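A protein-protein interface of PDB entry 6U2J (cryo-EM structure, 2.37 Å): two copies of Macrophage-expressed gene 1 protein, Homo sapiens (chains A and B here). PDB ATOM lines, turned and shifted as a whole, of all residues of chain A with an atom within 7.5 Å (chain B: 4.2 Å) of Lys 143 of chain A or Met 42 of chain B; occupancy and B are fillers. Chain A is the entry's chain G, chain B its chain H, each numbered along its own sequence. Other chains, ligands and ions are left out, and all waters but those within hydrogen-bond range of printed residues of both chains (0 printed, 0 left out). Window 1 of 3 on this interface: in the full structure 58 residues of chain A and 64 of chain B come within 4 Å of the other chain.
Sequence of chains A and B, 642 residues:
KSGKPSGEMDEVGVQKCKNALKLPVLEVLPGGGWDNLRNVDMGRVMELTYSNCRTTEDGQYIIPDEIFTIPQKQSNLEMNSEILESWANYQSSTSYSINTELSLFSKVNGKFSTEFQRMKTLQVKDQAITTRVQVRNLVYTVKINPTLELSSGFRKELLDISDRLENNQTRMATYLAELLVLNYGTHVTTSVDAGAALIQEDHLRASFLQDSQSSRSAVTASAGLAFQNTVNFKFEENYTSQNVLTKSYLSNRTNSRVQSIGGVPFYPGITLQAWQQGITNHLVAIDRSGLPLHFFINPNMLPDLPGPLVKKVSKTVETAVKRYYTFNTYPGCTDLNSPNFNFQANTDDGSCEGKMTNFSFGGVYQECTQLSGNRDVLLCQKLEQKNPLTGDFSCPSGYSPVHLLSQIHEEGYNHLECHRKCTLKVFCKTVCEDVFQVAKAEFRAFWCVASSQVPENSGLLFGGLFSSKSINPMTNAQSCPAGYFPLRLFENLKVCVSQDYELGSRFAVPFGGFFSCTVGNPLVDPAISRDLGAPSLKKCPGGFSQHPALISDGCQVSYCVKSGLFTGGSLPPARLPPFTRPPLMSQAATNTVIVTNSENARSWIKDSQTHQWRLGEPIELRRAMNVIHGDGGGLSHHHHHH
Among the printed residues, merely in contact across the chains: Ile 70 of chain A with Asp 41 of chain B (3.2 Å), Phe 68 of chain A with Gly 43 of chain B (3.6 Å), Lys 143 of chain A with Met 42 of chain B (3.6 Å), Pro 146 of chain A with Tyr 184 of chain B (3.6 Å) and Pro 146 of chain A with Asn 183 of chain B (3.6 Å).
No position is printed for both chains.
Of the 6 pairs that touch across the chains among the printed residues, none has its exchanged pair printed and touching as well.
The backbone carbonyl oxygen (O) of Phe 68 of chain A is in hydrogen-bond range of the backbone NH (N) of Lys 143 of chain A (3.0 Å).
O of Thr 141 of chain A sits at hydrogen-bond distance from N of Ile 70 of chain A, at 2.8 Å.
The backbone NH (N) of Met 42 of chain B sits at hydrogen-bond distance from the backbone carbonyl oxygen (O) of Gly 33 of chain B.
O of Gly 43 of chain B is in hydrogen-bond range of N of Gly 33 of chain B (2.5 Å).
The guanidinium group of Arg 38 of chain B lies close to the side-chain sulfur of Met 42 of chain B.
Printed residues of chain A that touch a printed residue of chain B: Phe 68, Ile 70, Lys 143 and Pro 146.
Hydrophobic or aromatic side chains of chain A within 4 Å of the printed part of chain B: Phe 68, Ile 70 and Pro 146.
Of the 12 printed residues of chain B, 5 touch a printed residue of chain A.
Printed residues of chain B that touch a printed residue of chain A: Asp 41, Met 42, Gly 43, Asn 183 and Tyr 184.
Hydrophobic or aromatic side chains of chain B that line the printed part of chain A: Met 42 and Tyr 184.
Among the printed residues, 6 pairs touch across the chains.
Among the printed residues, no Asp or Glu carboxylate lies within 4 Å of a Lys or Arg side-chain nitrogen of the other chain.
The side-chain amino group of Lys 143 of chain A lies within hydrogen-bond range of the backbone carbonyl oxygen of Asp 41 of chain B.
Of the printed residues of chain B, Ile 70 of chain A touches Asp 41.
Of the printed residues of chain B, Pro 146 of chain A touches Asn 183 (3.6 Å) and Tyr 184 (3.6 Å).
Val 192 of chain A touches none of the printed residues of chain B.
Of the printed residues of chain A, Asp 41 of chain B touches Ile 70 (3.2 Å) and Lys 143 (3.1 Å).
Met 42 of chain B touches just one residue of chain A: Lys 143 (3.6 Å).
Of chain A, only Phe 68 (3.6 Å) comes within 4 Å of Gly 43 of chain B.
Of the printed residues of chain A, Asn 183 of chain B touches Pro 146.
Of the printed residues of chain A, Tyr 184 of chain B touches Pro 146.
The nearest printed residue of chain B that does not touch Lys 143 of chain A is Val 40 of chain B (5.1 Å).
The nearest residue of chain A that does not touch Met 42 of chain B is Phe 68 of chain A (4.8 Å).
The nearest printed residue of chain A that does not touch Tyr 184 of chain B is Asn 145 of chain A (6.3 Å).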
ATOM      1  N   VAL A  28       6.714 -14.803   4.083  1.00  0.00           N
ATOM      2  CA  VAL A  28       5.717 -13.754   3.912  1.00  0.00           C
ATOM      3  C   VAL A  28       5.956 -12.737   5.019  1.00  0.00           C
ATOM      4  O   VAL A  28       5.522 -12.938   6.155  1.00  0.00           O
ATOM      5  CB  VAL A  28       4.292 -14.310   3.975  1.00  0.00           C
ATOM      6  CG1 VAL A  28       3.284 -13.234   3.672  1.00  0.00           C
ATOM      7  CG2 VAL A  28       4.142 -15.464   3.052  1.00  0.00           C
ATOM      8  N   LEU A  29       6.639 -11.637   4.708  1.00  0.00           N
ATOM      9  CA  LEU A  29       7.050 -10.723   5.762  1.00  0.00           C
ATOM     10  C   LEU A  29       6.615  -9.296   5.467  1.00  0.00           C
ATOM     11  O   LEU A  29       6.639  -8.862   4.314  1.00  0.00           O
ATOM     12  CB  LEU A  29       8.571 -10.762   5.954  1.00  0.00           C
ATOM     13  CG  LEU A  29       9.124 -12.101   6.441  1.00  0.00           C
ATOM     14  CD1 LEU A  29      10.626 -12.076   6.507  1.00  0.00           C
ATOM     15  CD2 LEU A  29       8.522 -12.473   7.779  1.00  0.00           C
ATOM     16  N   PRO A  30       6.205  -8.553   6.482  1.00  0.00           N
ATOM     17  CA  PRO A  30       5.870  -7.142   6.279  1.00  0.00           C
ATOM     18  C   PRO A  30       7.092  -6.249   6.401  1.00  0.00           C
ATOM     19  O   PRO A  30       8.209  -6.737   6.574  1.00  0.00           O
ATOM     20  CB  PRO A  30       4.854  -6.868   7.388  1.00  0.00           C
ATOM     21  CG  PRO A  30       5.246  -7.795   8.452  1.00  0.00           C
ATOM     22  CD  PRO A  30       5.789  -9.021   7.807  1.00  0.00           C
ATOM     23  N   GLY A  31       6.897  -4.941   6.298  1.00  0.00           N
ATOM     24  CA  GLY A  31       7.987  -4.002   6.366  1.00  0.00           C
ATOM     25  C   GLY A  31       8.602  -3.630   5.037  1.00  0.00           C
ATOM     26  O   GLY A  31       9.490  -2.775   5.006  1.00  0.00           O
ATOM     27  N   LEU A  48      15.028  -6.185   9.218  1.00  0.00           N
ATOM     28  CA  LEU A  48      14.620  -7.437   9.845  1.00  0.00           C
ATOM     29  C   LEU A  48      15.868  -8.268  10.114  1.00  0.00           C
ATOM     30  O   LEU A  48      16.507  -8.754   9.177  1.00  0.00           O
ATOM     31  CB  LEU A  48      13.625  -8.197   8.969  1.00  0.00           C
ATOM     32  CG  LEU A  48      12.285  -7.500   8.700  1.00  0.00           C
ATOM     33  CD1 LEU A  48      11.412  -8.336   7.799  1.00  0.00           C
ATOM     34  CD2 LEU A  48      11.548  -7.168   9.977  1.00  0.00           C
ATOM     35  N   GLU A  66      11.646  -8.804  15.382  1.00  0.00           N
ATOM     36  CA  GLU A  66      10.728  -7.690  15.561  1.00  0.00           C
ATOM     37  C   GLU A  66       9.430  -7.901  14.791  1.00  0.00           C
ATOM     38  O   GLU A  66       8.763  -6.947  14.391  1.00  0.00           O
ATOM     39  CB  GLU A  66      11.417  -6.392  15.156  1.00  0.00           C
ATOM     40  CG  GLU A  66      11.989  -6.404  13.754  1.00  0.00           C
ATOM     41  CD  GLU A  66      13.434  -6.885  13.696  1.00  0.00           C
ATOM     42  OE1 GLU A  66      13.897  -7.561  14.635  1.00  0.00           O
ATOM     43  OE2 GLU A  66      14.122  -6.561  12.715  1.00  0.00           O
ATOM     44  N   ILE A  67       9.059  -9.161  14.615  1.00  0.00           N
ATOM     45  CA  ILE A  67       7.854  -9.588  13.925  1.00  0.00           C
ATOM     46  C   ILE A  67       7.084 -10.486  14.878  1.00  0.00           C
ATOM     47  O   ILE A  67       7.672 -11.387  15.481  1.00  0.00           O
ATOM     48  CB  ILE A  67       8.210 -10.337  12.625  1.00  0.00           C
ATOM     49  CG1 ILE A  67       8.762  -9.378  11.575  1.00  0.00           C
ATOM     50  CG2 ILE A  67       7.066 -11.148  12.112  1.00  0.00           C
ATOM     51  CD1 ILE A  67       7.794  -8.346  11.149  1.00  0.00           C
ATOM     52  N   PHE A  68       5.788 -10.236  15.037  1.00  0.00           N
ATOM     53  CA  PHE A  68       4.938 -11.156  15.775  1.00  0.00           C
ATOM     54  C   PHE A  68       3.828 -11.671  14.870  1.00  0.00           C
ATOM     55  O   PHE A  68       3.271 -10.923  14.065  1.00  0.00           O
ATOM     56  CB  PHE A  68       4.366 -10.511  17.051  1.00  0.00           C
ATOM     57  CG  PHE A  68       3.365  -9.425  16.817  1.00  0.00           C
ATOM     58  CD1 PHE A  68       3.771  -8.128  16.570  1.00  0.00           C
ATOM     59  CD2 PHE A  68       2.010  -9.685  16.930  1.00  0.00           C
ATOM     60  CE1 PHE A  68       2.844  -7.125  16.384  1.00  0.00           C
ATOM     61  CE2 PHE A  68       1.082  -8.690  16.746  1.00  0.00           C
ATOM     62  CZ  PHE A  68       1.500  -7.408  16.474  1.00  0.00           C
ATOM     63  N   THR A  69       3.528 -12.958  14.998  1.00  0.00           N
ATOM     64  CA  THR A  69       2.506 -13.615  14.205  1.00  0.00           C
ATOM     65  C   THR A  69       1.293 -13.954  15.057  1.00  0.00           C
ATOM     66  O   THR A  69       1.390 -14.146  16.269  1.00  0.00           O
ATOM     67  CB  THR A  69       3.032 -14.895  13.553  1.00  0.00           C
ATOM     68  OG1 THR A  69       3.488 -15.793  14.567  1.00  0.00           O
ATOM     69  CG2 THR A  69       4.167 -14.582  12.610  1.00  0.00           C
ATOM     70  N   ILE A  70       0.147 -14.028  14.398  1.00  0.00           N
ATOM     71  CA  ILE A  70      -1.127 -14.360  15.014  1.00  0.00           C
ATOM     72  C   ILE A  70      -1.660 -15.595  14.300  1.00  0.00           C
ATOM     73  O   ILE A  70      -1.924 -15.541  13.099  1.00  0.00           O
ATOM     74  CB  ILE A  70      -2.125 -13.200  14.896  1.00  0.00           C
ATOM     75  CG1 ILE A  70      -1.553 -11.961  15.568  1.00  0.00           C
ATOM     76  CG2 ILE A  70      -3.438 -13.591  15.507  1.00  0.00           C
ATOM     77  CD1 ILE A  70      -2.117 -10.699  15.033  1.00  0.00           C
ATOM     78  N   GLN A  72      -4.121 -17.823  12.693  1.00  0.00           N
ATOM     79  CA  GLN A  72      -5.496 -17.745  12.229  1.00  0.00           C
ATOM     80  C   GLN A  72      -6.067 -19.116  11.913  1.00  0.00           C
ATOM     81  O   GLN A  72      -7.157 -19.444  12.382  1.00  0.00           O
ATOM     82  CB  GLN A  72      -5.580 -16.852  10.992  1.00  0.00           C
ATOM     83  CG  GLN A  72      -5.177 -15.425  11.229  1.00  0.00           C
ATOM     84  CD  GLN A  72      -6.146 -14.692  12.109  1.00  0.00           C
ATOM     85  OE1 GLN A  72      -7.344 -14.922  12.051  1.00  0.00           O
ATOM     86  NE2 GLN A  72      -5.639 -13.781  12.909  1.00  0.00           N
ATOM     87  N   TYR A 140      -1.607 -17.458   8.838  1.00  0.00           N
ATOM     88  CA  TYR A 140      -1.076 -16.525   9.821  1.00  0.00           C
ATOM     89  C   TYR A 140      -1.408 -15.099   9.425  1.00  0.00           C
ATOM     90  O   TYR A 140      -1.515 -14.777   8.244  1.00  0.00           O
ATOM     91  CB  TYR A 140       0.445 -16.602   9.957  1.00  0.00           C
ATOM     92  CG  TYR A 140       1.004 -17.927  10.361  1.00  0.00           C
ATOM     93  CD1 TYR A 140       0.953 -18.358  11.677  1.00  0.00           C
ATOM     94  CD2 TYR A 140       1.622 -18.737   9.428  1.00  0.00           C
ATOM     95  CE1 TYR A 140       1.475 -19.568  12.041  1.00  0.00           C
ATOM     96  CE2 TYR A 140       2.154 -19.940   9.782  1.00  0.00           C
ATOM     97  CZ  TYR A 140       2.073 -20.356  11.087  1.00  0.00           C
ATOM     98  OH  TYR A 140       2.602 -21.565  11.430  1.00  0.00           O
ATOM     99  N   THR A 141      -1.548 -14.244  10.425  1.00  0.00           N
ATOM    100  CA  THR A 141      -1.450 -12.804  10.250  1.00  0.00           C
ATOM    101  C   THR A 141      -0.105 -12.379  10.814  1.00  0.00           C
ATOM    102  O   THR A 141       0.220 -12.705  11.955  1.00  0.00           O
ATOM    103  CB  THR A 141      -2.594 -12.067  10.940  1.00  0.00           C
ATOM    104  OG1 THR A 141      -3.832 -12.433  10.331  1.00  0.00           O
ATOM    105  CG2 THR A 141      -2.418 -10.579  10.806  1.00  0.00           C
ATOM    106  N   VAL A 142       0.687 -11.684  10.008  1.00  0.00           N
ATOM    107  CA  VAL A 142       2.075 -11.392  10.331  1.00  0.00           C
ATOM    108  C   VAL A 142       2.226  -9.881  10.407  1.00  0.00           C
ATOM    109  O   VAL A 142       2.024  -9.190   9.406  1.00  0.00           O
ATOM    110  CB  VAL A 142       3.024 -11.992   9.283  1.00  0.00           C
ATOM    111  CG1 VAL A 142       4.419 -11.792   9.689  1.00  0.00           C
ATOM    112  CG2 VAL A 142       2.750 -13.464   9.080  1.00  0.00           C
ATOM    113  N   LYS A 143       2.579  -9.368  11.583  1.00  0.00           N
ATOM    114  CA  LYS A 143       2.644  -7.932  11.810  1.00  0.00           C
ATOM    115  C   LYS A 143       4.014  -7.492  12.302  1.00  0.00           C
ATOM    116  O   LYS A 143       4.802  -8.287  12.812  1.00  0.00           O
ATOM    117  CB  LYS A 143       1.608  -7.464  12.834  1.00  0.00           C
ATOM    118  CG  LYS A 143       0.185  -7.574  12.399  1.00  0.00           C
ATOM    119  CD  LYS A 143      -0.687  -6.779  13.333  1.00  0.00           C
ATOM    120  CE  LYS A 143      -2.105  -6.735  12.854  1.00  0.00           C
ATOM    121  NZ  LYS A 143      -2.790  -8.026  13.026  1.00  0.00           N
ATOM    122  N   ILE A 144       4.270  -6.196  12.167  1.00  0.00           N
ATOM    123  CA  ILE A 144       5.468  -5.557  12.700  1.00  0.00           C
ATOM    124  C   ILE A 144       5.169  -5.018  14.089  1.00  0.00           C
ATOM    125  O   ILE A 144       4.028  -4.694  14.424  1.00  0.00           O
ATOM    126  CB  ILE A 144       5.973  -4.426  11.778  1.00  0.00           C
ATOM    127  CG1 ILE A 144       4.894  -3.371  11.574  1.00  0.00           C
ATOM    128  CG2 ILE A 144       6.438  -4.953  10.458  1.00  0.00           C
ATOM    129  CD1 ILE A 144       5.379  -2.150  10.845  1.00  0.00           C
ATOM    130  N   ASN A 145       6.204  -4.930  14.908  1.00  0.00           N
ATOM    131  CA  ASN A 145       6.103  -4.229  16.173  1.00  0.00           C
ATOM    132  C   ASN A 145       6.108  -2.720  15.939  1.00  0.00           C
ATOM    133  O   ASN A 145       6.591  -2.249  14.906  1.00  0.00           O
ATOM    134  CB  ASN A 145       7.255  -4.624  17.091  1.00  0.00           C
ATOM    135  CG  ASN A 145       7.129  -6.036  17.603  1.00  0.00           C
ATOM    136  OD1 ASN A 145       7.964  -6.886  17.326  1.00  0.00           O
ATOM    137  ND2 ASN A 145       6.073  -6.294  18.360  1.00  0.00           N
ATOM    138  N   PRO A 146       5.539  -1.940  16.863  1.00  0.00           N
ATOM    139  CA  PRO A 146       5.615  -0.479  16.715  1.00  0.00           C
ATOM    140  C   PRO A 146       7.016   0.067  16.900  1.00  0.00           C
ATOM    141  O   PRO A 146       7.382   1.050  16.245  1.00  0.00           O
ATOM    142  CB  PRO A 146       4.668   0.032  17.804  1.00  0.00           C
ATOM    143  CG  PRO A 146       3.774  -1.104  18.084  1.00  0.00           C
ATOM    144  CD  PRO A 146       4.592  -2.325  17.920  1.00  0.00           C
ATOM    145  N   LEU A 148      10.476  -0.148  15.886  1.00  0.00           N
ATOM    146  CA  LEU A 148      11.112  -0.765  14.736  1.00  0.00           C
ATOM    147  C   LEU A 148      12.011   0.254  14.056  1.00  0.00           C
ATOM    148  O   LEU A 148      11.663   1.430  13.963  1.00  0.00           O
ATOM    149  CB  LEU A 148      10.054  -1.310  13.771  1.00  0.00           C
ATOM    150  CG  LEU A 148      10.468  -1.913  12.434  1.00  0.00           C
ATOM    151  CD1 LEU A 148      11.502  -2.981  12.620  1.00  0.00           C
ATOM    152  CD2 LEU A 148       9.248  -2.503  11.788  1.00  0.00           C
ATOM    153  N   THR A 189       4.068  -1.945   3.895  1.00  0.00           N
ATOM    154  CA  THR A 189       3.156  -2.940   4.441  1.00  0.00           C
ATOM    155  C   THR A 189       3.471  -3.164   5.912  1.00  0.00           C
ATOM    156  O   THR A 189       4.612  -3.458   6.271  1.00  0.00           O
ATOM    157  CB  THR A 189       3.251  -4.254   3.671  1.00  0.00           C
ATOM    158  OG1 THR A 189       4.547  -4.825   3.850  1.00  0.00           O
ATOM    159  CG2 THR A 189       3.028  -4.023   2.205  1.00  0.00           C
ATOM    160  N   THR A 190       2.462  -3.014   6.763  1.00  0.00           N
ATOM    161  CA  THR A 190       2.635  -3.249   8.187  1.00  0.00           C
ATOM    162  C   THR A 190       2.073  -4.585   8.642  1.00  0.00           C
ATOM    163  O   THR A 190       2.487  -5.083   9.691  1.00  0.00           O
ATOM    164  CB  THR A 190       1.984  -2.125   8.999  1.00  0.00           C
ATOM    165  OG1 THR A 190       0.583  -2.079   8.719  1.00  0.00           O
ATOM    166  CG2 THR A 190       2.607  -0.791   8.647  1.00  0.00           C
ATOM    167  N   SER A 191       1.158  -5.174   7.884  1.00  0.00           N
ATOM    168  CA  SER A 191       0.616  -6.484   8.204  1.00  0.00           C
ATOM    169  C   SER A 191       0.331  -7.223   6.912  1.00  0.00           C
ATOM    170  O   SER A 191      -0.184  -6.636   5.966  1.00  0.00           O
ATOM    171  CB  SER A 191      -0.660  -6.377   9.040  1.00  0.00           C
ATOM    172  OG  SER A 191      -1.704  -5.781   8.300  1.00  0.00           O
ATOM    173  N   VAL A 192       0.678  -8.504   6.871  1.00  0.00           N
ATOM    174  CA  VAL A 192       0.399  -9.356   5.725  1.00  0.00           C
ATOM    175  C   VAL A 192      -0.304 -10.622   6.193  1.00  0.00           C
ATOM    176  O   VAL A 192       0.022 -11.181   7.244  1.00  0.00           O
ATOM    177  CB  VAL A 192       1.673  -9.697   4.919  1.00  0.00           C
ATOM    178  CG1 VAL A 192       2.153  -8.491   4.162  1.00  0.00           C
ATOM    179  CG2 VAL A 192       2.781 -10.175   5.829  1.00  0.00           C
ATOM    180  N   ASP A 193      -1.284 -11.058   5.416  1.00  0.00           N
ATOM    181  CA  ASP A 193      -2.001 -12.307   5.642  1.00  0.00           C
ATOM    182  C   ASP A 193      -1.319 -13.408   4.841  1.00  0.00           C
ATOM    183  O   ASP A 193      -1.337 -13.384   3.612  1.00  0.00           O
ATOM    184  CB  ASP A 193      -3.466 -12.161   5.241  1.00  0.00           C
ATOM    185  CG  ASP A 193      -4.287 -11.417   6.276  1.00  0.00           C
ATOM    186  OD1 ASP A 193      -3.922 -11.444   7.468  1.00  0.00           O
ATOM    187  OD2 ASP A 193      -5.327 -10.830   5.912  1.00  0.00           O
ATOM    188  N   SER A 289      -2.132  -4.899   4.686  1.00  0.00           N
ATOM    189  CA  SER A 289      -2.475  -3.539   5.074  1.00  0.00           C
ATOM    190  C   SER A 289      -1.201  -2.728   5.231  1.00  0.00           C
ATOM    191  O   SER A 289      -0.105  -3.275   5.343  1.00  0.00           O
ATOM    192  CB  SER A 289      -3.275  -3.496   6.379  1.00  0.00           C
ATOM    193  OG  SER A 289      -4.562  -4.057   6.218  1.00  0.00           O
ATOM    194  N   GLY B  33      -3.069  -6.651  22.481  1.00  0.00           N
ATOM    195  CA  GLY B  33      -4.043  -5.621  22.219  1.00  0.00           C
ATOM    196  C   GLY B  33      -5.108  -6.066  21.247  1.00  0.00           C
ATOM    197  O   GLY B  33      -4.937  -7.001  20.476  1.00  0.00           O
ATOM    198  N   TRP B  34      -6.232  -5.365  21.277  1.00  0.00           N
ATOM    199  CA  TRP B  34      -7.398  -5.785  20.521  1.00  0.00           C
ATOM    200  C   TRP B  34      -8.159  -4.570  20.032  1.00  0.00           C
ATOM    201  O   TRP B  34      -8.510  -3.699  20.827  1.00  0.00           O
ATOM    202  CB  TRP B  34      -8.300  -6.657  21.390  1.00  0.00           C
ATOM    203  CG  TRP B  34      -9.530  -7.139  20.728  1.00  0.00           C
ATOM    204  CD1 TRP B  34     -10.786  -6.675  20.916  1.00  0.00           C
ATOM    205  CD2 TRP B  34      -9.629  -8.194  19.776  1.00  0.00           C
ATOM    206  NE1 TRP B  34     -11.666  -7.373  20.142  1.00  0.00           N
ATOM    207  CE2 TRP B  34     -10.979  -8.311  19.429  1.00  0.00           C
ATOM    208  CE3 TRP B  34      -8.707  -9.048  19.183  1.00  0.00           C
ATOM    209  CZ2 TRP B  34     -11.432  -9.259  18.534  1.00  0.00           C
ATOM    210  CZ3 TRP B  34      -9.155  -9.973  18.276  1.00  0.00           C
ATOM    211  CH2 TRP B  34     -10.498 -10.058  17.944  1.00  0.00           C
ATOM    212  N   ASP B  35      -8.413  -4.520  18.732  1.00  0.00           N
ATOM    213  CA  ASP B  35      -9.257  -3.494  18.140  1.00  0.00           C
ATOM    214  C   ASP B  35     -10.691  -3.999  18.137  1.00  0.00           C
ATOM    215  O   ASP B  35     -11.014  -4.952  17.426  1.00  0.00           O
ATOM    216  CB  ASP B  35      -8.780  -3.164  16.727  1.00  0.00           C
ATOM    217  CG  ASP B  35      -9.555  -2.028  16.084  1.00  0.00           C
ATOM    218  OD1 ASP B  35     -10.562  -1.572  16.646  1.00  0.00           O
ATOM    219  OD2 ASP B  35      -9.134  -1.568  15.010  1.00  0.00           O
ATOM    220  N   ARG B  38     -12.814  -3.539  14.500  1.00  0.00           N
ATOM    221  CA  ARG B  38     -12.486  -4.379  13.364  1.00  0.00           C
ATOM    222  C   ARG B  38     -12.318  -5.842  13.731  1.00  0.00           C
ATOM    223  O   ARG B  38     -12.169  -6.669  12.828  1.00  0.00           O
ATOM    224  CB  ARG B  38     -11.196  -3.889  12.709  1.00  0.00           C
ATOM    225  CG  ARG B  38     -11.253  -2.488  12.157  1.00  0.00           C
ATOM    226  CD  ARG B  38      -9.931  -2.152  11.516  1.00  0.00           C
ATOM    227  NE  ARG B  38      -8.859  -2.093  12.497  1.00  0.00           N
ATOM    228  CZ  ARG B  38      -7.572  -2.111  12.188  1.00  0.00           C
ATOM    229  NH1 ARG B  38      -7.201  -2.211  10.923  1.00  0.00           N
ATOM    230  NH2 ARG B  38      -6.658  -2.053  13.141  1.00  0.00           N
ATOM    231  N   VAL B  40      -9.645  -7.294  15.284  1.00  0.00           N
ATOM    232  CA  VAL B  40      -8.309  -7.751  14.929  1.00  0.00           C
ATOM    233  C   VAL B  40      -7.398  -7.628  16.141  1.00  0.00           C
ATOM    234  O   VAL B  40      -7.655  -6.852  17.064  1.00  0.00           O
ATOM    235  CB  VAL B  40      -7.706  -6.984  13.728  1.00  0.00           C
ATOM    236  CG1 VAL B  40      -8.568  -7.134  12.499  1.00  0.00           C
ATOM    237  CG2 VAL B  40      -7.505  -5.529  14.050  1.00  0.00           C
ATOM    238  N   ASP B  41      -6.327  -8.414  16.131  1.00  0.00           N
ATOM    239  CA  ASP B  41      -5.308  -8.360  17.168  1.00  0.00           C
ATOM    240  C   ASP B  41      -4.316  -7.249  16.868  1.00  0.00           C
ATOM    241  O   ASP B  41      -3.874  -7.095  15.731  1.00  0.00           O
ATOM    242  CB  ASP B  41      -4.587  -9.697  17.272  1.00  0.00           C
ATOM    243  CG  ASP B  41      -5.441 -10.773  17.876  1.00  0.00           C
ATOM    244  OD1 ASP B  41      -6.199 -10.477  18.808  1.00  0.00           O
ATOM    245  OD2 ASP B  41      -5.378 -11.922  17.399  1.00  0.00           O
ATOM    246  N   MET B  42      -3.968  -6.475  17.892  1.00  0.00           N
ATOM    247  CA  MET B  42      -3.218  -5.229  17.740  1.00  0.00           C
ATOM    248  C   MET B  42      -2.086  -5.162  18.754  1.00  0.00           C
ATOM    249  O   MET B  42      -2.234  -4.487  19.766  1.00  0.00           O
ATOM    250  CB  MET B  42      -4.164  -4.046  17.925  1.00  0.00           C
ATOM    251  CG  MET B  42      -5.079  -3.703  16.775  1.00  0.00           C
ATOM    252  SD  MET B  42      -4.209  -2.807  15.486  1.00  0.00           S
ATOM    253  CE  MET B  42      -4.057  -4.061  14.249  1.00  0.00           C
ATOM    254  N   GLY B  43      -0.951  -5.797  18.482  1.00  0.00           N
ATOM    255  CA  GLY B  43       0.224  -5.557  19.312  1.00  0.00           C
ATOM    256  C   GLY B  43       0.211  -6.107  20.731  1.00  0.00           C
ATOM    257  O   GLY B  43      -0.840  -6.442  21.276  1.00  0.00           O
ATOM    258  N   LEU B 182      -3.679   3.230  17.438  1.00  0.00           N
ATOM    259  CA  LEU B 182      -3.421   2.623  16.138  1.00  0.00           C
ATOM    260  C   LEU B 182      -2.554   1.380  16.266  1.00  0.00           C
ATOM    261  O   LEU B 182      -2.767   0.392  15.558  1.00  0.00           O
ATOM    262  CB  LEU B 182      -2.754   3.637  15.211  1.00  0.00           C
ATOM    263  CG  LEU B 182      -2.399   3.162  13.802  1.00  0.00           C
ATOM    264  CD1 LEU B 182      -3.646   2.822  13.018  1.00  0.00           C
ATOM    265  CD2 LEU B 182      -1.560   4.191  13.075  1.00  0.00           C
ATOM    266  N   ASN B 183      -1.598   1.398  17.183  1.00  0.00           N
ATOM    267  CA  ASN B 183      -0.685   0.281  17.338  1.00  0.00           C
ATOM    268  C   ASN B 183      -1.190  -0.778  18.302  1.00  0.00           C
ATOM    269  O   ASN B 183      -0.879  -1.958  18.125  1.00  0.00           O
ATOM    270  CB  ASN B 183       0.673   0.781  17.822  1.00  0.00           C
ATOM    271  CG  ASN B 183       1.393   1.602  16.781  1.00  0.00           C
ATOM    272  OD1 ASN B 183       1.340   1.303  15.593  1.00  0.00           O
ATOM    273  ND2 ASN B 183       2.089   2.636  17.227  1.00  0.00           N
ATOM    274  N   TYR B 184      -1.954  -0.395  19.323  1.00  0.00           N
ATOM    275  CA  TYR B 184      -2.320  -1.322  20.380  1.00  0.00           C
ATOM    276  C   TYR B 184      -3.815  -1.521  20.556  1.00  0.00           C
ATOM    277  O   TYR B 184      -4.213  -2.268  21.451  1.00  0.00           O
ATOM    278  CB  TYR B 184      -1.702  -0.883  21.709  1.00  0.00           C
ATOM    279  CG  TYR B 184      -0.209  -1.020  21.719  1.00  0.00           C
ATOM    280  CD1 TYR B 184       0.388  -2.241  21.970  1.00  0.00           C
ATOM    281  CD2 TYR B 184       0.606   0.066  21.451  1.00  0.00           C
ATOM    282  CE1 TYR B 184       1.752  -2.374  21.971  1.00  0.00           C
ATOM    283  CE2 TYR B 184       1.972  -0.060  21.444  1.00  0.00           C
ATOM    284  CZ  TYR B 184       2.539  -1.281  21.707  1.00  0.00           C
ATOM    285  OH  TYR B 184       3.899  -1.413  21.706  1.00  0.00           O
ATOM    286  N   GLY B 185      -4.645  -0.904  19.741  1.00  0.00           N
ATOM    287  CA  GLY B 185      -6.062  -1.167  19.804  1.00  0.00           C
ATOM    288  C   GLY B 185      -6.752  -0.446  20.944  1.00  0.00           C
ATOM    289  O   GLY B 185      -6.219   0.463  21.570  1.00  0.00           O
